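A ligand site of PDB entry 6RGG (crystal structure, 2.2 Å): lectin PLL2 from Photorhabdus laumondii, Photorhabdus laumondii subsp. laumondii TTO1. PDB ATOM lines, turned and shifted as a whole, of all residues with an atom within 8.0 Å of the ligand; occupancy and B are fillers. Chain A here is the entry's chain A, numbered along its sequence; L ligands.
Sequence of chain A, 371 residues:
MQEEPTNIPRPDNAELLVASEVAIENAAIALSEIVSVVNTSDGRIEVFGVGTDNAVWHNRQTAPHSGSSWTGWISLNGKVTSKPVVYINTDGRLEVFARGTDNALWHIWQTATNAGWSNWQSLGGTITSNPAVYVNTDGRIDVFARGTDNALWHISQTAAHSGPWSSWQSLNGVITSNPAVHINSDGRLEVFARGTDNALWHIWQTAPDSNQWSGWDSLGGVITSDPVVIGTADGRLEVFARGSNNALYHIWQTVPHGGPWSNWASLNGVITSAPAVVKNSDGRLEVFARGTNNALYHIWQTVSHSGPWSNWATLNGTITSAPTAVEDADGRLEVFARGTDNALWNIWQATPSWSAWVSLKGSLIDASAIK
OG1 of Thr 101 lies within hydrogen-bond range of O4 of the ligand (3.0 Å). An oxygen (O4) of the ligand sits at hydrogen-bond distance from the backbone NH (N) of Thr 101 (3.5 Å). An oxygen (O6) of the ligand lies within hydrogen-bond range of the backbone NH of Lys 79 (3.0 Å).
The backbone carbonyl oxygen of Asn 54 lies within hydrogen-bond range of the backbone NH of Val 80 (2.9 Å). The side-chain carboxylate (OD1) of Asp 102 sits at hydrogen-bond distance from the indole nitrogen (NE1) of Trp 106 (3.1 Å). The backbone carbonyl oxygen (O) of Ala 98 sits at hydrogen-bond distance from the backbone NH (N) of Trp 106, 2.8 Å away. The backbone carbonyl oxygen (O) of Leu 76 sits at hydrogen-bond distance from the indole nitrogen (NE1) of Trp 120 (3.0 Å). The backbone carbonyl oxygen of Asn 77 lies within hydrogen-bond range of the indole nitrogen of Trp 120 (3.5 Å).
Merely in contact with the ligand: Gly 78 (3.2 Å), Trp 120 (3.5 Å), Trp 106 (3.7 Å) and Val 80 (3.7 Å). The nearest printed residue that does not touch the ligand is Gly 100 (4.1 Å).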
ATOM      1  N   ASN A  54      27.019 -15.595 -24.056  1.00  0.00           N
ATOM      2  CA  ASN A  54      25.899 -14.607 -24.116  1.00  0.00           C
ATOM      3  C   ASN A  54      24.738 -15.134 -24.978  1.00  0.00           C
ATOM      4  O   ASN A  54      23.848 -14.345 -25.356  1.00  0.00           O
ATOM      5  CB  ASN A  54      26.376 -13.220 -24.593  1.00  0.00           C
ATOM      6  CG  ASN A  54      27.048 -12.457 -23.469  1.00  0.00           C
ATOM      7  OD1 ASN A  54      28.192 -12.724 -23.151  1.00  0.00           O
ATOM      8  ND2 ASN A  54      26.328 -11.540 -22.851  1.00  0.00           N
ATOM      9  N   ALA A  55      24.683 -16.435 -25.250  1.00  0.00           N
ATOM     10  CA  ALA A  55      23.486 -17.073 -25.849  1.00  0.00           C
ATOM     11  C   ALA A  55      22.538 -17.402 -24.700  1.00  0.00           C
ATOM     12  O   ALA A  55      22.995 -17.362 -23.517  1.00  0.00           O
ATOM     13  CB  ALA A  55      23.865 -18.296 -26.643  1.00  0.00           C
ATOM     14  N   VAL A  56      21.271 -17.645 -25.038  1.00  0.00           N
ATOM     15  CA  VAL A  56      20.234 -18.146 -24.094  1.00  0.00           C
ATOM     16  C   VAL A  56      20.293 -19.659 -24.176  1.00  0.00           C
ATOM     17  O   VAL A  56      20.240 -20.176 -25.292  1.00  0.00           O
ATOM     18  CB  VAL A  56      18.824 -17.594 -24.408  1.00  0.00           C
ATOM     19  CG1 VAL A  56      17.737 -18.298 -23.607  1.00  0.00           C
ATOM     20  CG2 VAL A  56      18.732 -16.093 -24.167  1.00  0.00           C
ATOM     21  N   LEU A  76      19.680 -21.871 -27.496  1.00  0.00           N
ATOM     22  CA  LEU A  76      18.814 -21.127 -28.434  1.00  0.00           C
ATOM     23  C   LEU A  76      19.631 -20.060 -29.162  1.00  0.00           C
ATOM     24  O   LEU A  76      19.051 -19.340 -29.994  1.00  0.00           O
ATOM     25  CB  LEU A  76      17.663 -20.517 -27.627  1.00  0.00           C
ATOM     26  CG  LEU A  76      16.651 -21.531 -27.116  1.00  0.00           C
ATOM     27  CD1 LEU A  76      15.663 -20.866 -26.176  1.00  0.00           C
ATOM     28  CD2 LEU A  76      15.930 -22.213 -28.275  1.00  0.00           C
ATOM     29  N   ASN A  77      20.943 -19.982 -28.909  1.00  0.00           N
ATOM     30  CA  ASN A  77      21.845 -19.076 -29.668  1.00  0.00           C
ATOM     31  C   ASN A  77      21.470 -17.649 -29.282  1.00  0.00           C
ATOM     32  O   ASN A  77      21.013 -17.441 -28.152  1.00  0.00           O
ATOM     33  CB  ASN A  77      21.771 -19.331 -31.182  1.00  0.00           C
ATOM     34  CG  ASN A  77      21.922 -20.780 -31.606  1.00  0.00           C
ATOM     35  OD1 ASN A  77      21.054 -21.345 -32.275  1.00  0.00           O
ATOM     36  ND2 ASN A  77      23.031 -21.405 -31.230  1.00  0.00           N
ATOM     37  N   GLY A  78      21.606 -16.690 -30.197  1.00  0.00           N
ATOM     38  CA  GLY A  78      21.351 -15.271 -29.925  1.00  0.00           C
ATOM     39  C   GLY A  78      22.471 -14.670 -29.107  1.00  0.00           C
ATOM     40  O   GLY A  78      23.355 -15.409 -28.689  1.00  0.00           O
ATOM     41  N   LYS A  79      22.452 -13.351 -28.930  1.00  0.00           N
ATOM     42  CA  LYS A  79      23.457 -12.573 -28.176  1.00  0.00           C
ATOM     43  C   LYS A  79      22.682 -11.575 -27.323  1.00  0.00           C
ATOM     44  O   LYS A  79      22.048 -10.688 -27.903  1.00  0.00           O
ATOM     45  CB  LYS A  79      24.429 -11.863 -29.133  1.00  0.00           C
ATOM     46  CG  LYS A  79      25.534 -12.732 -29.713  1.00  0.00           C
ATOM     47  CD  LYS A  79      26.759 -12.860 -28.824  1.00  0.00           C
ATOM     48  CE  LYS A  79      27.561 -11.576 -28.650  1.00  0.00           C
ATOM     49  NZ  LYS A  79      28.816 -11.792 -27.876  1.00  0.00           N
ATOM     50  N   VAL A  80      22.677 -11.754 -25.999  1.00  0.00           N
ATOM     51  CA  VAL A  80      21.719 -11.042 -25.104  1.00  0.00           C
ATOM     52  C   VAL A  80      22.511 -10.307 -24.028  1.00  0.00           C
ATOM     53  O   VAL A  80      23.588 -10.796 -23.647  1.00  0.00           O
ATOM     54  CB  VAL A  80      20.655 -12.003 -24.539  1.00  0.00           C
ATOM     55  CG1 VAL A  80      20.033 -12.854 -25.651  1.00  0.00           C
ATOM     56  CG2 VAL A  80      21.188 -12.882 -23.434  1.00  0.00           C
ATOM     57  N   THR A  81      21.989  -9.148 -23.620  1.00  0.00           N
ATOM     58  CA  THR A  81      22.600  -8.232 -22.615  1.00  0.00           C
ATOM     59  C   THR A  81      21.599  -7.984 -21.476  1.00  0.00           C
ATOM     60  O   THR A  81      21.747  -6.978 -20.771  1.00  0.00           O
ATOM     61  CB  THR A  81      23.070  -6.931 -23.284  1.00  0.00           C
ATOM     62  OG1 THR A  81      21.994  -6.415 -24.082  1.00  0.00           O
ATOM     63  CG2 THR A  81      24.299  -7.136 -24.155  1.00  0.00           C
ATOM     64  N   VAL A  96      10.480 -16.547 -25.264  1.00  0.00           N
ATOM     65  CA  VAL A  96      11.560 -15.916 -24.478  1.00  0.00           C
ATOM     66  C   VAL A  96      11.826 -14.517 -25.049  1.00  0.00           C
ATOM     67  O   VAL A  96      11.884 -14.382 -26.272  1.00  0.00           O
ATOM     68  CB  VAL A  96      12.810 -16.813 -24.488  1.00  0.00           C
ATOM     69  CG1 VAL A  96      13.924 -16.226 -23.655  1.00  0.00           C
ATOM     70  CG2 VAL A  96      12.472 -18.215 -24.036  1.00  0.00           C
ATOM     71  N   PHE A  97      11.999 -13.547 -24.166  1.00  0.00           N
ATOM     72  CA  PHE A  97      12.244 -12.124 -24.454  1.00  0.00           C
ATOM     73  C   PHE A  97      13.563 -11.735 -23.795  1.00  0.00           C
ATOM     74  O   PHE A  97      13.814 -12.200 -22.694  1.00  0.00           O
ATOM     75  CB  PHE A  97      11.072 -11.294 -23.911  1.00  0.00           C
ATOM     76  CG  PHE A  97       9.765 -11.606 -24.580  1.00  0.00           C
ATOM     77  CD1 PHE A  97       9.398 -10.964 -25.744  1.00  0.00           C
ATOM     78  CD2 PHE A  97       8.924 -12.581 -24.073  1.00  0.00           C
ATOM     79  CE1 PHE A  97       8.216 -11.292 -26.387  1.00  0.00           C
ATOM     80  CE2 PHE A  97       7.741 -12.908 -24.716  1.00  0.00           C
ATOM     81  CZ  PHE A  97       7.396 -12.261 -25.879  1.00  0.00           C
ATOM     82  N   ALA A  98      14.384 -10.915 -24.462  1.00  0.00           N
ATOM     83  CA  ALA A  98      15.736 -10.514 -23.992  1.00  0.00           C
ATOM     84  C   ALA A  98      16.199  -9.269 -24.735  1.00  0.00           C
ATOM     85  O   ALA A  98      15.846  -9.124 -25.927  1.00  0.00           O
ATOM     86  CB  ALA A  98      16.723 -11.644 -24.211  1.00  0.00           C
ATOM     87  N   ARG A  99      16.996  -8.437 -24.076  1.00  0.00           N
ATOM     88  CA  ARG A  99      17.694  -7.312 -24.726  1.00  0.00           C
ATOM     89  C   ARG A  99      18.818  -7.886 -25.591  1.00  0.00           C
ATOM     90  O   ARG A  99      19.565  -8.758 -25.085  1.00  0.00           O
ATOM     91  CB  ARG A  99      18.198  -6.312 -23.677  1.00  0.00           C
ATOM     92  CG  ARG A  99      18.808  -5.069 -24.297  1.00  0.00           C
ATOM     93  CD  ARG A  99      19.127  -3.980 -23.281  1.00  0.00           C
ATOM     94  NE  ARG A  99      20.281  -4.352 -22.499  1.00  0.00           N
ATOM     95  CZ  ARG A  99      20.899  -3.536 -21.677  1.00  0.00           C
ATOM     96  NH1 ARG A  99      20.465  -2.305 -21.527  1.00  0.00           N
ATOM     97  NH2 ARG A  99      21.962  -3.960 -20.999  1.00  0.00           N
ATOM     98  N   GLY A 100      18.900  -7.476 -26.855  1.00  0.00           N
ATOM     99  CA  GLY A 100      19.996  -7.836 -27.781  1.00  0.00           C
ATOM    100  C   GLY A 100      21.246  -6.990 -27.539  1.00  0.00           C
ATOM    101  O   GLY A 100      21.231  -6.172 -26.589  1.00  0.00           O
ATOM    102  N   THR A 101      22.298  -7.177 -28.343  1.00  0.00           N
ATOM    103  CA  THR A 101      23.580  -6.418 -28.247  1.00  0.00           C
ATOM    104  C   THR A 101      23.374  -4.990 -28.751  1.00  0.00           C
ATOM    105  O   THR A 101      24.142  -4.136 -28.342  1.00  0.00           O
ATOM    106  CB  THR A 101      24.711  -7.077 -29.041  1.00  0.00           C
ATOM    107  OG1 THR A 101      24.265  -7.373 -30.366  1.00  0.00           O
ATOM    108  CG2 THR A 101      25.214  -8.331 -28.372  1.00  0.00           C
ATOM    109  N   ASP A 102      22.395  -4.778 -29.646  1.00  0.00           N
ATOM    110  CA  ASP A 102      21.930  -3.441 -30.118  1.00  0.00           C
ATOM    111  C   ASP A 102      21.047  -2.761 -29.055  1.00  0.00           C
ATOM    112  O   ASP A 102      20.650  -1.625 -29.285  1.00  0.00           O
ATOM    113  CB  ASP A 102      21.205  -3.557 -31.459  1.00  0.00           C
ATOM    114  CG  ASP A 102      20.080  -4.594 -31.508  1.00  0.00           C
ATOM    115  OD1 ASP A 102      19.674  -5.076 -30.414  1.00  0.00           O
ATOM    116  OD2 ASP A 102      19.616  -4.924 -32.656  1.00  0.00           O
ATOM    117  N   ASN A 103      20.707  -3.438 -27.949  1.00  0.00           N
ATOM    118  CA  ASN A 103      19.872  -2.909 -26.838  1.00  0.00           C
ATOM    119  C   ASN A 103      18.392  -2.814 -27.249  1.00  0.00           C
ATOM    120  O   ASN A 103      17.605  -2.211 -26.488  1.00  0.00           O
ATOM    121  CB  ASN A 103      20.444  -1.589 -26.312  1.00  0.00           C
ATOM    122  CG  ASN A 103      21.690  -1.790 -25.475  1.00  0.00           C
ATOM    123  OD1 ASN A 103      22.086  -2.925 -25.186  1.00  0.00           O
ATOM    124  ND2 ASN A 103      22.319  -0.707 -25.084  1.00  0.00           N
ATOM    125  N   ALA A 104      17.994  -3.410 -28.371  1.00  0.00           N
ATOM    126  CA  ALA A 104      16.584  -3.616 -28.766  1.00  0.00           C
ATOM    127  C   ALA A 104      16.030  -4.834 -28.015  1.00  0.00           C
ATOM    128  O   ALA A 104      16.838  -5.625 -27.469  1.00  0.00           O
ATOM    129  CB  ALA A 104      16.465  -3.805 -30.271  1.00  0.00           C
ATOM    130  N   LEU A 105      14.708  -4.981 -27.998  1.00  0.00           N
ATOM    131  CA  LEU A 105      14.037  -6.185 -27.440  1.00  0.00           C
ATOM    132  C   LEU A 105      13.988  -7.234 -28.544  1.00  0.00           C
ATOM    133  O   LEU A 105      13.463  -6.944 -29.609  1.00  0.00           O
ATOM    134  CB  LEU A 105      12.629  -5.836 -26.947  1.00  0.00           C
ATOM    135  CG  LEU A 105      11.817  -7.011 -26.408  1.00  0.00           C
ATOM    136  CD1 LEU A 105      12.391  -7.502 -25.094  1.00  0.00           C
ATOM    137  CD2 LEU A 105      10.368  -6.625 -26.236  1.00  0.00           C
ATOM    138  N   TRP A 106      14.522  -8.420 -28.271  1.00  0.00           N
ATOM    139  CA  TRP A 106      14.427  -9.593 -29.168  1.00  0.00           C
ATOM    140  C   TRP A 106      13.498 -10.633 -28.529  1.00  0.00           C
ATOM    141  O   TRP A 106      13.325 -10.591 -27.309  1.00  0.00           O
ATOM    142  CB  TRP A 106      15.832 -10.133 -29.447  1.00  0.00           C
ATOM    143  CG  TRP A 106      16.649  -9.214 -30.304  1.00  0.00           C
ATOM    144  CD1 TRP A 106      17.214  -8.029 -29.934  1.00  0.00           C
ATOM    145  CD2 TRP A 106      16.961  -9.400 -31.684  1.00  0.00           C
ATOM    146  NE1 TRP A 106      17.876  -7.470 -31.000  1.00  0.00           N
ATOM    147  CE2 TRP A 106      17.740  -8.301 -32.086  1.00  0.00           C
ATOM    148  CE3 TRP A 106      16.686 -10.414 -32.615  1.00  0.00           C
ATOM    149  CZ2 TRP A 106      18.226  -8.172 -33.384  1.00  0.00           C
ATOM    150  CZ3 TRP A 106      17.175 -10.299 -33.899  1.00  0.00           C
ATOM    151  CH2 TRP A 106      17.942  -9.191 -34.275  1.00  0.00           C
ATOM    152  N   HIS A 107      12.965 -11.560 -29.329  1.00  0.00           N
ATOM    153  CA  HIS A 107      12.152 -12.678 -28.804  1.00  0.00           C
ATOM    154  C   HIS A 107      12.268 -13.892 -29.727  1.00  0.00           C
ATOM    155  O   HIS A 107      12.693 -13.737 -30.862  1.00  0.00           O
ATOM    156  CB  HIS A 107      10.689 -12.242 -28.589  1.00  0.00           C
ATOM    157  CG  HIS A 107       9.886 -12.076 -29.833  1.00  0.00           C
ATOM    158  ND1 HIS A 107       8.622 -12.602 -29.954  1.00  0.00           N
ATOM    159  CD2 HIS A 107      10.136 -11.422 -30.985  1.00  0.00           C
ATOM    160  CE1 HIS A 107       8.133 -12.300 -31.135  1.00  0.00           C
ATOM    161  NE2 HIS A 107       9.041 -11.564 -31.780  1.00  0.00           N
ATOM    162  N   ILE A 108      11.858 -15.042 -29.223  1.00  0.00           N
ATOM    163  CA  ILE A 108      11.955 -16.360 -29.896  1.00  0.00           C
ATOM    164  C   ILE A 108      10.934 -17.267 -29.209  1.00  0.00           C
ATOM    165  O   ILE A 108      10.713 -17.115 -27.994  1.00  0.00           O
ATOM    166  CB  ILE A 108      13.407 -16.894 -29.810  1.00  0.00           C
ATOM    167  CG1 ILE A 108      13.564 -18.266 -30.481  1.00  0.00           C
ATOM    168  CG2 ILE A 108      13.913 -16.899 -28.376  1.00  0.00           C
ATOM    169  CD1 ILE A 108      15.014 -18.687 -30.646  1.00  0.00           C
ATOM    170  N   TRP A 120      15.320 -16.144 -33.795  1.00  0.00           N
ATOM    171  CA  TRP A 120      15.223 -14.867 -33.049  1.00  0.00           C
ATOM    172  C   TRP A 120      14.663 -13.795 -33.986  1.00  0.00           C
ATOM    173  O   TRP A 120      14.983 -13.832 -35.179  1.00  0.00           O
ATOM    174  CB  TRP A 120      16.591 -14.446 -32.503  1.00  0.00           C
ATOM    175  CG  TRP A 120      17.023 -15.148 -31.257  1.00  0.00           C
ATOM    176  CD1 TRP A 120      17.925 -16.173 -31.148  1.00  0.00           C
ATOM    177  CD2 TRP A 120      16.633 -14.808 -29.917  1.00  0.00           C
ATOM    178  NE1 TRP A 120      18.107 -16.498 -29.836  1.00  0.00           N
ATOM    179  CE2 TRP A 120      17.331 -15.677 -29.052  1.00  0.00           C
ATOM    180  CE3 TRP A 120      15.755 -13.868 -29.365  1.00  0.00           C
ATOM    181  CZ2 TRP A 120      17.158 -15.634 -27.668  1.00  0.00           C
ATOM    182  CZ3 TRP A 120      15.610 -13.805 -27.998  1.00  0.00           C
ATOM    183  CH2 TRP A 120      16.298 -14.687 -27.160  1.00  0.00           C
ATOM    184  N   GLN A 121      13.876 -12.867 -33.442  1.00  0.00           N
ATOM    185  CA  GLN A 121      13.247 -11.776 -34.207  1.00  0.00           C
ATOM    186  C   GLN A 121      13.244 -10.548 -33.299  1.00  0.00           C
ATOM    187  O   GLN A 121      13.077 -10.739 -32.078  1.00  0.00           O
ATOM    188  CB  GLN A 121      11.856 -12.147 -34.707  1.00  0.00           C
ATOM    189  CG  GLN A 121      11.183 -11.046 -35.509  1.00  0.00           C
ATOM    190  CD  GLN A 121       9.715 -11.320 -35.781  1.00  0.00           C
ATOM    191  OE1 GLN A 121       8.825 -10.683 -35.209  1.00  0.00           O
ATOM    192  NE2 GLN A 121       9.465 -12.278 -36.646  1.00  0.00           N
ATOM    193  N   SER A 122      13.489  -9.381 -33.889  1.00  0.00           N
ATOM    194  CA  SER A 122      13.587  -8.068 -33.199  1.00  0.00           C
ATOM    195  C   SER A 122      12.216  -7.411 -33.130  1.00  0.00           C
ATOM    196  O   SER A 122      11.439  -7.501 -34.119  1.00  0.00           O
ATOM    197  CB  SER A 122      14.582  -7.152 -33.870  1.00  0.00           C
ATOM    198  OG  SER A 122      14.719  -5.933 -33.142  1.00  0.00           O
HETATM  199  C1  LIG L   1      22.336 -12.713 -33.416  1.00  0.00           C
HETATM  200  O1  LIG L   1      22.303 -13.862 -34.289  1.00  0.00           O
HETATM  201  C2  LIG L   1      22.810 -11.426 -34.102  1.00  0.00           C
HETATM  202  O2  LIG L   1      24.079 -11.696 -34.682  1.00  0.00           O
HETATM  203  O3  LIG L   1      21.053 -12.421 -32.884  1.00  0.00           O
HETATM  204  C3  LIG L   1      21.247 -11.495 -31.800  1.00  0.00           C
HETATM  205  C4  LIG L   1      21.732 -10.109 -32.250  1.00  0.00           C
HETATM  206  O4  LIG L   1      21.998  -9.250 -31.095  1.00  0.00           O
HETATM  207  C5  LIG L   1      22.970 -10.243 -33.137  1.00  0.00           C
HETATM  208  O5  LIG L   1      23.185  -9.004 -33.835  1.00  0.00           O
HETATM  209  C6  LIG L   1      19.965 -11.365 -31.010  1.00  0.00           C
HETATM  210  O6  LIG L   1      19.861 -12.490 -30.161  1.00  0.00           O
HETATM  211  C7  LIG L   1      24.551  -8.705 -34.162  1.00  0.00           C
HETATM  212  C8  LIG L   1      18.895 -12.223 -29.145  1.00  0.00           C
